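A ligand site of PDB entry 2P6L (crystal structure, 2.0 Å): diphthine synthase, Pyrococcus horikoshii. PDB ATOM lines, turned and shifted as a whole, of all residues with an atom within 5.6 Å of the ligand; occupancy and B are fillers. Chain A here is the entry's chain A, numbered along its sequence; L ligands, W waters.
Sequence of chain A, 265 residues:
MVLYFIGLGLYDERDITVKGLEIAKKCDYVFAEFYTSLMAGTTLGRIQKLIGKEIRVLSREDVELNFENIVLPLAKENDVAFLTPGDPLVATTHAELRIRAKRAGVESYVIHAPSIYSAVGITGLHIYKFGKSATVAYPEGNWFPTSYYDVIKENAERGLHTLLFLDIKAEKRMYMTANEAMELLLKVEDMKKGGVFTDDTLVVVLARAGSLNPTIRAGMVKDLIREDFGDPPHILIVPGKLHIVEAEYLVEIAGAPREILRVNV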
ATOM      1  N   LEU A  10     -11.574 -12.067 -33.247  1.00  0.00           N
ATOM      2  CA  LEU A  10     -10.378 -11.216 -33.200  1.00  0.00           C
ATOM      3  C   LEU A  10     -10.586  -9.748 -33.659  1.00  0.00           C
ATOM      4  O   LEU A  10     -10.026  -8.828 -33.089  1.00  0.00           O
ATOM      5  CB  LEU A  10      -9.328 -11.830 -34.126  1.00  0.00           C
ATOM      6  CG  LEU A  10      -8.843 -13.204 -33.675  1.00  0.00           C
ATOM      7  CD1 LEU A  10      -8.132 -13.942 -34.798  1.00  0.00           C
ATOM      8  CD2 LEU A  10      -7.830 -13.114 -32.523  1.00  0.00           C
ATOM      9  N   TYR A  11     -11.336  -9.548 -34.779  1.00  0.00           N
ATOM     10  CA  TYR A  11     -11.314  -8.226 -35.438  1.00  0.00           C
ATOM     11  C   TYR A  11     -12.712  -7.594 -35.624  1.00  0.00           C
ATOM     12  O   TYR A  11     -12.974  -6.468 -35.216  1.00  0.00           O
ATOM     13  CB  TYR A  11     -10.635  -8.398 -36.806  1.00  0.00           C
ATOM     14  CG  TYR A  11     -10.415  -7.065 -37.421  1.00  0.00           C
ATOM     15  CD1 TYR A  11      -9.587  -6.132 -36.794  1.00  0.00           C
ATOM     16  CD2 TYR A  11     -11.019  -6.733 -38.639  1.00  0.00           C
ATOM     17  CE1 TYR A  11      -9.360  -4.900 -37.378  1.00  0.00           C
ATOM     18  CE2 TYR A  11     -10.799  -5.494 -39.214  1.00  0.00           C
ATOM     19  CZ  TYR A  11      -9.984  -4.582 -38.592  1.00  0.00           C
ATOM     20  OH  TYR A  11      -9.758  -3.344 -39.161  1.00  0.00           O
ATOM     21  N   THR A  36     -11.998  -6.165 -22.165  1.00  0.00           N
ATOM     22  CA  THR A  36     -10.942  -7.174 -22.093  1.00  0.00           C
ATOM     23  C   THR A  36     -10.068  -7.199 -23.343  1.00  0.00           C
ATOM     24  O   THR A  36      -8.979  -7.768 -23.346  1.00  0.00           O
ATOM     25  CB  THR A  36     -11.518  -8.583 -21.852  1.00  0.00           C
ATOM     26  OG1 THR A  36     -12.466  -8.910 -22.888  1.00  0.00           O
ATOM     27  CG2 THR A  36     -12.202  -8.647 -20.498  1.00  0.00           C
ATOM     28  N   SER A  37     -10.557  -6.577 -24.415  1.00  0.00           N
ATOM     29  CA  SER A  37      -9.807  -6.542 -25.653  1.00  0.00           C
ATOM     30  C   SER A  37     -10.437  -5.528 -26.599  1.00  0.00           C
ATOM     31  O   SER A  37     -11.490  -4.958 -26.295  1.00  0.00           O
ATOM     32  CB  SER A  37      -9.803  -7.928 -26.313  1.00  0.00           C
ATOM     33  OG  SER A  37      -8.892  -7.965 -27.398  1.00  0.00           O
ATOM     34  N   LEU A  38      -9.806  -5.317 -27.749  1.00  0.00           N
ATOM     35  CA  LEU A  38     -10.317  -4.379 -28.732  1.00  0.00           C
ATOM     36  C   LEU A  38     -10.582  -5.041 -30.073  1.00  0.00           C
ATOM     37  O   LEU A  38      -9.708  -5.683 -30.644  1.00  0.00           O
ATOM     38  CB  LEU A  38      -9.319  -3.224 -28.927  1.00  0.00           C
ATOM     39  CG  LEU A  38      -9.607  -2.228 -30.060  1.00  0.00           C
ATOM     40  CD1 LEU A  38     -10.880  -1.459 -29.777  1.00  0.00           C
ATOM     41  CD2 LEU A  38      -8.426  -1.280 -30.214  1.00  0.00           C
ATOM     42  N   PRO A  85     -14.948 -10.080 -26.708  1.00  0.00           N
ATOM     43  CA  PRO A  85     -14.031 -10.100 -27.855  1.00  0.00           C
ATOM     44  C   PRO A  85     -13.238 -11.416 -27.790  1.00  0.00           C
ATOM     45  O   PRO A  85     -13.120 -12.011 -26.718  1.00  0.00           O
ATOM     46  CB  PRO A  85     -13.137  -8.889 -27.606  1.00  0.00           C
ATOM     47  CG  PRO A  85     -14.017  -7.967 -26.810  1.00  0.00           C
ATOM     48  CD  PRO A  85     -14.711  -8.906 -25.863  1.00  0.00           C
ATOM     49  N   GLY A  86     -12.703 -11.873 -28.920  1.00  0.00           N
ATOM     50  CA  GLY A  86     -11.930 -13.099 -28.961  1.00  0.00           C
ATOM     51  C   GLY A  86     -12.672 -14.268 -28.320  1.00  0.00           C
ATOM     52  O   GLY A  86     -13.865 -14.426 -28.533  1.00  0.00           O
ATOM     53  N   ASP A  87     -11.941 -15.103 -27.576  1.00  0.00           N
ATOM     54  CA  ASP A  87     -12.543 -16.239 -26.869  1.00  0.00           C
ATOM     55  C   ASP A  87     -12.834 -15.729 -25.458  1.00  0.00           C
ATOM     56  O   ASP A  87     -11.968 -15.143 -24.811  1.00  0.00           O
ATOM     57  CB  ASP A  87     -11.582 -17.424 -26.822  1.00  0.00           C
ATOM     58  CG  ASP A  87     -12.180 -18.622 -26.118  1.00  0.00           C
ATOM     59  OD1 ASP A  87     -12.412 -18.546 -24.888  1.00  0.00           O
ATOM     60  OD2 ASP A  87     -12.419 -19.658 -26.785  1.00  0.00           O
ATOM     61  N   PRO A  88     -14.059 -15.958 -24.948  1.00  0.00           N
ATOM     62  CA  PRO A  88     -14.454 -15.496 -23.614  1.00  0.00           C
ATOM     63  C   PRO A  88     -13.611 -15.904 -22.400  1.00  0.00           C
ATOM     64  O   PRO A  88     -13.564 -15.167 -21.416  1.00  0.00           O
ATOM     65  CB  PRO A  88     -15.901 -15.984 -23.496  1.00  0.00           C
ATOM     66  CG  PRO A  88     -15.938 -17.185 -24.382  1.00  0.00           C
ATOM     67  CD  PRO A  88     -15.130 -16.763 -25.572  1.00  0.00           C
ATOM     68  N   LEU A  89     -12.937 -17.042 -22.482  1.00  0.00           N
ATOM     69  CA  LEU A  89     -12.145 -17.525 -21.346  1.00  0.00           C
ATOM     70  C   LEU A  89     -10.633 -17.352 -21.437  1.00  0.00           C
ATOM     71  O   LEU A  89      -9.907 -17.717 -20.517  1.00  0.00           O
ATOM     72  CB  LEU A  89     -12.461 -19.001 -21.100  1.00  0.00           C
ATOM     73  CG  LEU A  89     -13.944 -19.393 -21.145  1.00  0.00           C
ATOM     74  CD1 LEU A  89     -14.090 -20.859 -20.782  1.00  0.00           C
ATOM     75  CD2 LEU A  89     -14.734 -18.537 -20.164  1.00  0.00           C
ATOM     76  N   VAL A  90     -10.154 -16.799 -22.547  1.00  0.00           N
ATOM     77  CA  VAL A  90      -8.727 -16.621 -22.751  1.00  0.00           C
ATOM     78  C   VAL A  90      -8.190 -15.271 -22.273  1.00  0.00           C
ATOM     79  O   VAL A  90      -8.589 -14.214 -22.763  1.00  0.00           O
ATOM     80  CB  VAL A  90      -8.361 -16.771 -24.239  1.00  0.00           C
ATOM     81  CG1 VAL A  90      -6.888 -16.439 -24.461  1.00  0.00           C
ATOM     82  CG2 VAL A  90      -8.681 -18.191 -24.712  1.00  0.00           C
ATOM     83  N   ALA A  91      -7.280 -15.323 -21.306  1.00  0.00           N
ATOM     84  CA  ALA A  91      -6.670 -14.113 -20.759  1.00  0.00           C
ATOM     85  C   ALA A  91      -7.686 -13.154 -20.163  1.00  0.00           C
ATOM     86  O   ALA A  91      -7.558 -11.938 -20.309  1.00  0.00           O
ATOM     87  CB  ALA A  91      -5.845 -13.419 -21.836  1.00  0.00           C
ATOM     88  N   THR A  92      -8.697 -13.707 -19.520  1.00  0.00           N
ATOM     89  CA  THR A  92      -9.722 -12.939 -18.838  1.00  0.00           C
ATOM     90  C   THR A  92      -9.966 -13.729 -17.571  1.00  0.00           C
ATOM     91  O   THR A  92      -9.361 -14.784 -17.371  1.00  0.00           O
ATOM     92  CB  THR A  92     -11.045 -12.874 -19.618  1.00  0.00           C
ATOM     93  OG1 THR A  92     -11.656 -14.175 -19.625  1.00  0.00           O
ATOM     94  CG2 THR A  92     -10.821 -12.405 -21.047  1.00  0.00           C
ATOM     95  N   PRO A 114     -12.282 -17.391 -32.594  1.00  0.00           N
ATOM     96  CA  PRO A 114     -10.832 -17.244 -32.756  1.00  0.00           C
ATOM     97  C   PRO A 114     -10.207 -16.346 -31.687  1.00  0.00           C
ATOM     98  O   PRO A 114     -10.742 -15.288 -31.359  1.00  0.00           O
ATOM     99  CB  PRO A 114     -10.685 -16.689 -34.176  1.00  0.00           C
ATOM    100  CG  PRO A 114     -12.038 -16.091 -34.490  1.00  0.00           C
ATOM    101  CD  PRO A 114     -13.001 -17.031 -33.831  1.00  0.00           C
ATOM    102  N   SER A 115      -9.065 -16.782 -31.148  1.00  0.00           N
ATOM    103  CA  SER A 115      -8.363 -16.076 -30.082  1.00  0.00           C
ATOM    104  C   SER A 115      -6.968 -15.650 -30.510  1.00  0.00           C
ATOM    105  O   SER A 115      -6.326 -16.313 -31.325  1.00  0.00           O
ATOM    106  CB  SER A 115      -8.244 -16.985 -28.855  1.00  0.00           C
ATOM    107  OG  SER A 115      -7.486 -16.378 -27.825  1.00  0.00           O
ATOM    108  N   ILE A 116      -6.492 -14.543 -29.959  1.00  0.00           N
ATOM    109  CA  ILE A 116      -5.157 -14.067 -30.285  1.00  0.00           C
ATOM    110  C   ILE A 116      -4.134 -15.124 -29.865  1.00  0.00           C
ATOM    111  O   ILE A 116      -3.056 -15.228 -30.451  1.00  0.00           O
ATOM    112  CB  ILE A 116      -4.832 -12.725 -29.570  1.00  0.00           C
ATOM    113  CG1 ILE A 116      -3.511 -12.153 -30.095  1.00  0.00           C
ATOM    114  CG2 ILE A 116      -4.740 -12.938 -28.052  1.00  0.00           C
ATOM    115  CD1 ILE A 116      -3.551 -11.761 -31.571  1.00  0.00           C
ATOM    116  N   TYR A 117      -4.497 -15.928 -28.872  1.00  0.00           N
ATOM    117  CA  TYR A 117      -3.589 -16.964 -28.371  1.00  0.00           C
ATOM    118  C   TYR A 117      -3.204 -18.002 -29.432  1.00  0.00           C
ATOM    119  O   TYR A 117      -2.091 -18.521 -29.422  1.00  0.00           O
ATOM    120  CB  TYR A 117      -4.208 -17.660 -27.159  1.00  0.00           C
ATOM    121  CG  TYR A 117      -3.207 -18.497 -26.376  1.00  0.00           C
ATOM    122  CD1 TYR A 117      -2.194 -17.887 -25.630  1.00  0.00           C
ATOM    123  CD2 TYR A 117      -3.274 -19.889 -26.405  1.00  0.00           C
ATOM    124  CE1 TYR A 117      -1.276 -18.657 -24.922  1.00  0.00           C
ATOM    125  CE2 TYR A 117      -2.356 -20.659 -25.697  1.00  0.00           C
ATOM    126  CZ  TYR A 117      -1.358 -20.036 -24.962  1.00  0.00           C
ATOM    127  OH  TYR A 117      -0.468 -20.818 -24.257  1.00  0.00           O
ATOM    128  N   LEU A 164       3.355 -11.855 -25.382  1.00  0.00           N
ATOM    129  CA  LEU A 164       3.093 -10.743 -24.478  1.00  0.00           C
ATOM    130  C   LEU A 164       1.816  -9.999 -24.812  1.00  0.00           C
ATOM    131  O   LEU A 164       1.770  -9.230 -25.778  1.00  0.00           O
ATOM    132  CB  LEU A 164       4.265  -9.760 -24.497  1.00  0.00           C
ATOM    133  CG  LEU A 164       5.643 -10.308 -24.096  1.00  0.00           C
ATOM    134  CD1 LEU A 164       6.728  -9.290 -24.412  1.00  0.00           C
ATOM    135  CD2 LEU A 164       5.624 -10.665 -22.609  1.00  0.00           C
ATOM    136  N   PHE A 165       0.769 -10.241 -24.023  1.00  0.00           N
ATOM    137  CA  PHE A 165      -0.492  -9.538 -24.206  1.00  0.00           C
ATOM    138  C   PHE A 165      -0.152  -8.105 -23.812  1.00  0.00           C
ATOM    139  O   PHE A 165       0.676  -7.892 -22.923  1.00  0.00           O
ATOM    140  CB  PHE A 165      -1.546 -10.091 -23.240  1.00  0.00           C
ATOM    141  CG  PHE A 165      -1.936 -11.522 -23.508  1.00  0.00           C
ATOM    142  CD1 PHE A 165      -2.849 -11.826 -24.501  1.00  0.00           C
ATOM    143  CD2 PHE A 165      -1.404 -12.554 -22.742  1.00  0.00           C
ATOM    144  CE1 PHE A 165      -3.253 -13.163 -24.736  1.00  0.00           C
ATOM    145  CE2 PHE A 165      -1.786 -13.891 -22.969  1.00  0.00           C
ATOM    146  CZ  PHE A 165      -2.714 -14.187 -23.960  1.00  0.00           C
ATOM    147  N   LEU A 166      -0.766  -7.123 -24.458  1.00  0.00           N
ATOM    148  CA  LEU A 166      -0.465  -5.740 -24.120  1.00  0.00           C
ATOM    149  C   LEU A 166      -1.608  -5.115 -23.329  1.00  0.00           C
ATOM    150  O   LEU A 166      -2.773  -5.478 -23.512  1.00  0.00           O
ATOM    151  CB  LEU A 166      -0.158  -4.944 -25.394  1.00  0.00           C
ATOM    152  CG  LEU A 166       1.023  -5.510 -26.199  1.00  0.00           C
ATOM    153  CD1 LEU A 166       1.477  -4.477 -27.240  1.00  0.00           C
ATOM    154  CD2 LEU A 166       2.179  -5.836 -25.269  1.00  0.00           C
ATOM    155  N   ASP A 167      -1.276  -4.181 -22.457  1.00  0.00           N
ATOM    156  CA  ASP A 167      -2.277  -3.553 -21.609  1.00  0.00           C
ATOM    157  C   ASP A 167      -3.380  -2.772 -22.325  1.00  0.00           C
ATOM    158  O   ASP A 167      -3.219  -2.324 -23.473  1.00  0.00           O
ATOM    159  CB  ASP A 167      -1.590  -2.640 -20.573  1.00  0.00           C
ATOM    160  CG  ASP A 167      -2.337  -2.606 -19.250  1.00  0.00           C
ATOM    161  OD1 ASP A 167      -3.422  -3.222 -19.145  1.00  0.00           O
ATOM    162  OD2 ASP A 167      -1.845  -1.941 -18.309  1.00  0.00           O
ATOM    163  N   ILE A 168      -4.503  -2.627 -21.639  1.00  0.00           N
ATOM    164  CA  ILE A 168      -5.631  -1.898 -22.177  1.00  0.00           C
ATOM    165  C   ILE A 168      -6.422  -1.227 -21.057  1.00  0.00           C
ATOM    166  O   ILE A 168      -6.631  -1.812 -19.990  1.00  0.00           O
ATOM    167  CB  ILE A 168      -6.564  -2.848 -22.991  1.00  0.00           C
ATOM    168  CG1 ILE A 168      -7.894  -2.162 -23.281  1.00  0.00           C
ATOM    169  CG2 ILE A 168      -6.764  -4.155 -22.244  1.00  0.00           C
ATOM    170  CD1 ILE A 168      -8.829  -2.985 -24.140  1.00  0.00           C
ATOM    171  N   LEU A 206       2.489  -8.379 -34.035  1.00  0.00           N
ATOM    172  CA  LEU A 206       1.284  -8.774 -34.741  1.00  0.00           C
ATOM    173  C   LEU A 206       0.214  -7.763 -34.342  1.00  0.00           C
ATOM    174  O   LEU A 206      -0.115  -7.629 -33.160  1.00  0.00           O
ATOM    175  CB  LEU A 206       0.850 -10.191 -34.328  1.00  0.00           C
ATOM    176  CG  LEU A 206      -0.466 -10.729 -34.887  1.00  0.00           C
ATOM    177  CD1 LEU A 206      -0.477 -10.663 -36.419  1.00  0.00           C
ATOM    178  CD2 LEU A 206      -0.665 -12.156 -34.417  1.00  0.00           C
ATOM    179  N   ALA A 207      -0.291  -7.021 -35.329  1.00  0.00           N
ATOM    180  CA  ALA A 207      -1.297  -6.008 -35.071  1.00  0.00           C
ATOM    181  C   ALA A 207      -2.581  -6.286 -35.844  1.00  0.00           C
ATOM    182  O   ALA A 207      -2.545  -6.595 -37.033  1.00  0.00           O
ATOM    183  CB  ALA A 207      -0.762  -4.620 -35.434  1.00  0.00           C
ATOM    184  N   ARG A 208      -3.709  -6.176 -35.146  1.00  0.00           N
ATOM    185  CA  ARG A 208      -5.026  -6.392 -35.740  1.00  0.00           C
ATOM    186  C   ARG A 208      -5.193  -7.761 -36.392  1.00  0.00           C
ATOM    187  O   ARG A 208      -5.638  -7.878 -37.532  1.00  0.00           O
ATOM    188  CB  ARG A 208      -5.322  -5.284 -36.754  1.00  0.00           C
ATOM    189  CG  ARG A 208      -5.187  -3.875 -36.178  1.00  0.00           C
ATOM    190  CD  ARG A 208      -5.430  -2.812 -37.242  1.00  0.00           C
ATOM    191  NE  ARG A 208      -4.584  -3.037 -38.415  1.00  0.00           N
ATOM    192  CZ  ARG A 208      -3.273  -2.837 -38.435  1.00  0.00           C
ATOM    193  NH1 ARG A 208      -2.630  -2.396 -37.362  1.00  0.00           N
ATOM    194  NH2 ARG A 208      -2.580  -3.102 -39.543  1.00  0.00           N
ATOM    195  N   ALA A 209      -4.810  -8.804 -35.663  1.00  0.00           N
ATOM    196  CA  ALA A 209      -4.971 -10.155 -36.155  1.00  0.00           C
ATOM    197  C   ALA A 209      -6.472 -10.279 -36.419  1.00  0.00           C
ATOM    198  O   ALA A 209      -7.282  -9.641 -35.740  1.00  0.00           O
ATOM    199  CB  ALA A 209      -4.532 -11.171 -35.097  1.00  0.00           C
ATOM    200  N   GLY A 210      -6.862 -11.080 -37.407  1.00  0.00           N
ATOM    201  CA  GLY A 210      -8.276 -11.223 -37.692  1.00  0.00           C
ATOM    202  C   GLY A 210      -8.688 -10.384 -38.889  1.00  0.00           C
ATOM    203  O   GLY A 210      -9.629 -10.709 -39.594  1.00  0.00           O
ATOM    204  N   PRO A 233      -5.566  -3.359 -31.811  1.00  0.00           N
ATOM    205  CA  PRO A 233      -4.663  -3.916 -30.794  1.00  0.00           C
ATOM    206  C   PRO A 233      -3.386  -4.542 -31.361  1.00  0.00           C
ATOM    207  O   PRO A 233      -3.348  -4.974 -32.518  1.00  0.00           O
ATOM    208  CB  PRO A 233      -5.535  -4.941 -30.103  1.00  0.00           C
ATOM    209  CG  PRO A 233      -6.310  -5.505 -31.252  1.00  0.00           C
ATOM    210  CD  PRO A 233      -6.707  -4.269 -32.044  1.00  0.00           C
ATOM    211  N   HIS A 234      -2.356  -4.583 -30.517  1.00  0.00           N
ATOM    212  CA  HIS A 234      -1.075  -5.164 -30.873  1.00  0.00           C
ATOM    213  C   HIS A 234      -0.686  -6.182 -29.821  1.00  0.00           C
ATOM    214  O   HIS A 234      -1.172  -6.136 -28.698  1.00  0.00           O
ATOM    215  CB  HIS A 234       0.050  -4.108 -30.870  1.00  0.00           C
ATOM    216  CG  HIS A 234      -0.127  -2.976 -31.828  1.00  0.00           C
ATOM    217  ND1 HIS A 234       0.749  -1.914 -31.871  1.00  0.00           N
ATOM    218  CD2 HIS A 234      -1.065  -2.735 -32.771  1.00  0.00           C
ATOM    219  CE1 HIS A 234       0.357  -1.064 -32.808  1.00  0.00           C
ATOM    220  NE2 HIS A 234      -0.736  -1.544 -33.369  1.00  0.00           N
ATOM    221  N   ILE A 235       0.207  -7.089 -30.188  1.00  0.00           N
ATOM    222  CA  ILE A 235       0.761  -8.042 -29.253  1.00  0.00           C
ATOM    223  C   ILE A 235       2.230  -8.061 -29.601  1.00  0.00           C
ATOM    224  O   ILE A 235       2.602  -7.796 -30.746  1.00  0.00           O
ATOM    225  CB  ILE A 235       0.231  -9.492 -29.377  1.00  0.00           C
ATOM    226  CG1 ILE A 235       0.512 -10.048 -30.772  1.00  0.00           C
ATOM    227  CG2 ILE A 235      -1.227  -9.530 -29.008  1.00  0.00           C
ATOM    228  CD1 ILE A 235       0.532 -11.569 -30.801  1.00  0.00           C
HETATM  229  N1  LIG L   1      -9.970 -13.293 -24.786  1.00  0.00           N
HETATM  230  C1  LIG L   1      -9.103 -12.506 -25.742  1.00  0.00           C
HETATM  231  C2  LIG L   1      -7.842 -11.889 -25.181  1.00  0.00           C
HETATM  232  C3  LIG L   1      -7.967 -10.915 -24.011  1.00  0.00           C
HETATM  233  S1  LIG L   1      -6.322 -10.108 -23.772  1.00  0.00           S
HETATM  234  C4  LIG L   1      -8.771 -13.489 -26.941  1.00  0.00           C
HETATM  235  O1  LIG L   1      -9.208 -14.651 -26.913  1.00  0.00           O
HETATM  236  O2  LIG L   1      -8.046 -13.003 -27.898  1.00  0.00           O
HETATM  237  C5  LIG L   1      -6.444  -8.642 -24.718  1.00  0.00           C
HETATM  238  C6  LIG L   1      -5.033  -8.336 -25.349  1.00  0.00           C
HETATM  239  O3  LIG L   1      -4.718  -9.394 -26.282  1.00  0.00           O
HETATM  240  C7  LIG L   1      -4.930  -7.055 -26.101  1.00  0.00           C
HETATM  241  O4  LIG L   1      -4.623  -5.973 -25.246  1.00  0.00           O
HETATM  242  C8  LIG L   1      -3.836  -7.392 -27.149  1.00  0.00           C
HETATM  243  O5  LIG L   1      -2.495  -7.204 -26.673  1.00  0.00           O
HETATM  244  C9  LIG L   1      -4.181  -8.854 -27.588  1.00  0.00           C
HETATM  245  N2  LIG L   1      -5.106  -8.985 -28.650  1.00  0.00           N
HETATM  246  C10 LIG L   1      -6.444  -9.322 -28.705  1.00  0.00           C
HETATM  247  N3  LIG L   1      -6.967  -9.325 -29.900  1.00  0.00           N
HETATM  248  C11 LIG L   1      -5.900  -8.967 -30.760  1.00  0.00           C
HETATM  249  C12 LIG L   1      -5.833  -8.800 -32.191  1.00  0.00           C
HETATM  250  N4  LIG L   1      -6.883  -8.984 -33.016  1.00  0.00           N
HETATM  251  N5  LIG L   1      -4.603  -8.432 -32.676  1.00  0.00           N
HETATM  252  C13 LIG L   1      -3.512  -8.227 -31.876  1.00  0.00           C
HETATM  253  N6  LIG L   1      -3.531  -8.383 -30.509  1.00  0.00           N
HETATM  254  C14 LIG L   1      -4.761  -8.742 -30.021  1.00  0.00           C
HETATM  255  O   HOH W   1      -4.424  -3.318 -26.049  1.00  0.00           O
HETATM  256  O   HOH W   2     -11.595 -10.925 -24.577  1.00  0.00           O
HETATM  257  O   HOH W   3     -10.186  -8.711 -29.771  1.00  0.00           O
HETATM  258  O   HOH W   4      -9.407 -11.151 -29.822  1.00  0.00           O
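O5 of the ligand lies within hydrogen-bond range of N of Leu 166, at 2.8 Å. O of Leu 166 lies within hydrogen-bond range of O4 of the ligand, 2.6 Å away. OG of Ser 115 is in hydrogen-bond range of O1 of the ligand, at 2.6 Å. The backbone carbonyl oxygen (O) of Val 90 lies within hydrogen-bond range of a nitrogen (N1) of the ligand, 2.6 Å away. The backbone carbonyl oxygen (O) of His 234 is in hydrogen-bond range of an oxygen (O5) of the ligand. O1 of the ligand sits at hydrogen-bond distance from N of Asp 87, at 2.8 Å. The backbone carbonyl oxygen of Asp 87 is in hydrogen-bond range of a nitrogen (N1) of the ligand (2.7 Å). N of Ala 209 is in hydrogen-bond range of N5 of the ligand, 3.0 Å away. The backbone carbonyl oxygen (O) of Ala 209 is in hydrogen-bond range of a nitrogen (N4) of the ligand, at 2.8 Å. The backbone NH of Ile 116 lies within hydrogen-bond range of an oxygen (O2) of the ligand (3.0 Å). A nitrogen (N3) of the ligand sits close to the side-chain hydroxyl of Ser 37 (3.4 Å). The backbone carbonyl oxygen (O) of Leu 10 sits at hydrogen-bond distance from a nitrogen (N4) of the ligand (3.1 Å). A nitrogen (N5) of the ligand is in hydrogen-bond range of the backbone NH of Arg 208, 3.5 Å away.
The side-chain hydroxyl (OG) of Ser 115 sits close to the backbone NH (N) of Tyr 117 (3.2 Å). OD1 of Asp 87 sits at hydrogen-bond distance from N of Leu 89. N of Ile 235 sits at hydrogen-bond distance from O of Leu 206. The backbone carbonyl oxygen (O) of Pro 233 sits at hydrogen-bond distance from the backbone NH (N) of Arg 208, 2.9 Å away. O of Pro 88 lies within hydrogen-bond range of OG1 of Thr 92.
Water W1 lies within hydrogen-bond range of an oxygen (O4) of the ligand (2.8 Å) and the backbone carbonyl oxygen (O) of Asp 167 (3.0 Å). Water W2 lies within hydrogen-bond range of the side-chain hydroxyl (OG1) of Thr 36 (2.8 Å), the backbone carbonyl oxygen (O) of Pro 85 (2.8 Å) and a nitrogen (N1) of the ligand (2.9 Å). Water W4 bridges O2 of the ligand and N of Gly 86.
The backbone carbonyl oxygen of Thr 36 sits close to a sulfur (S1) of the ligand (3.6 Å). Residues that only touch the ligand: Ile 235 (3.0 Å), Pro 233 (3.3 Å), Phe 165 (3.5 Å), Leu 206 (3.7 Å), Gly 86 (3.7 Å), Ala 91 (3.9 Å), Pro 85 (3.9 Å) and Thr 92 (3.9 Å). The nearest printed residue that does not touch the ligand is Ile 168 (4.1 Å).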
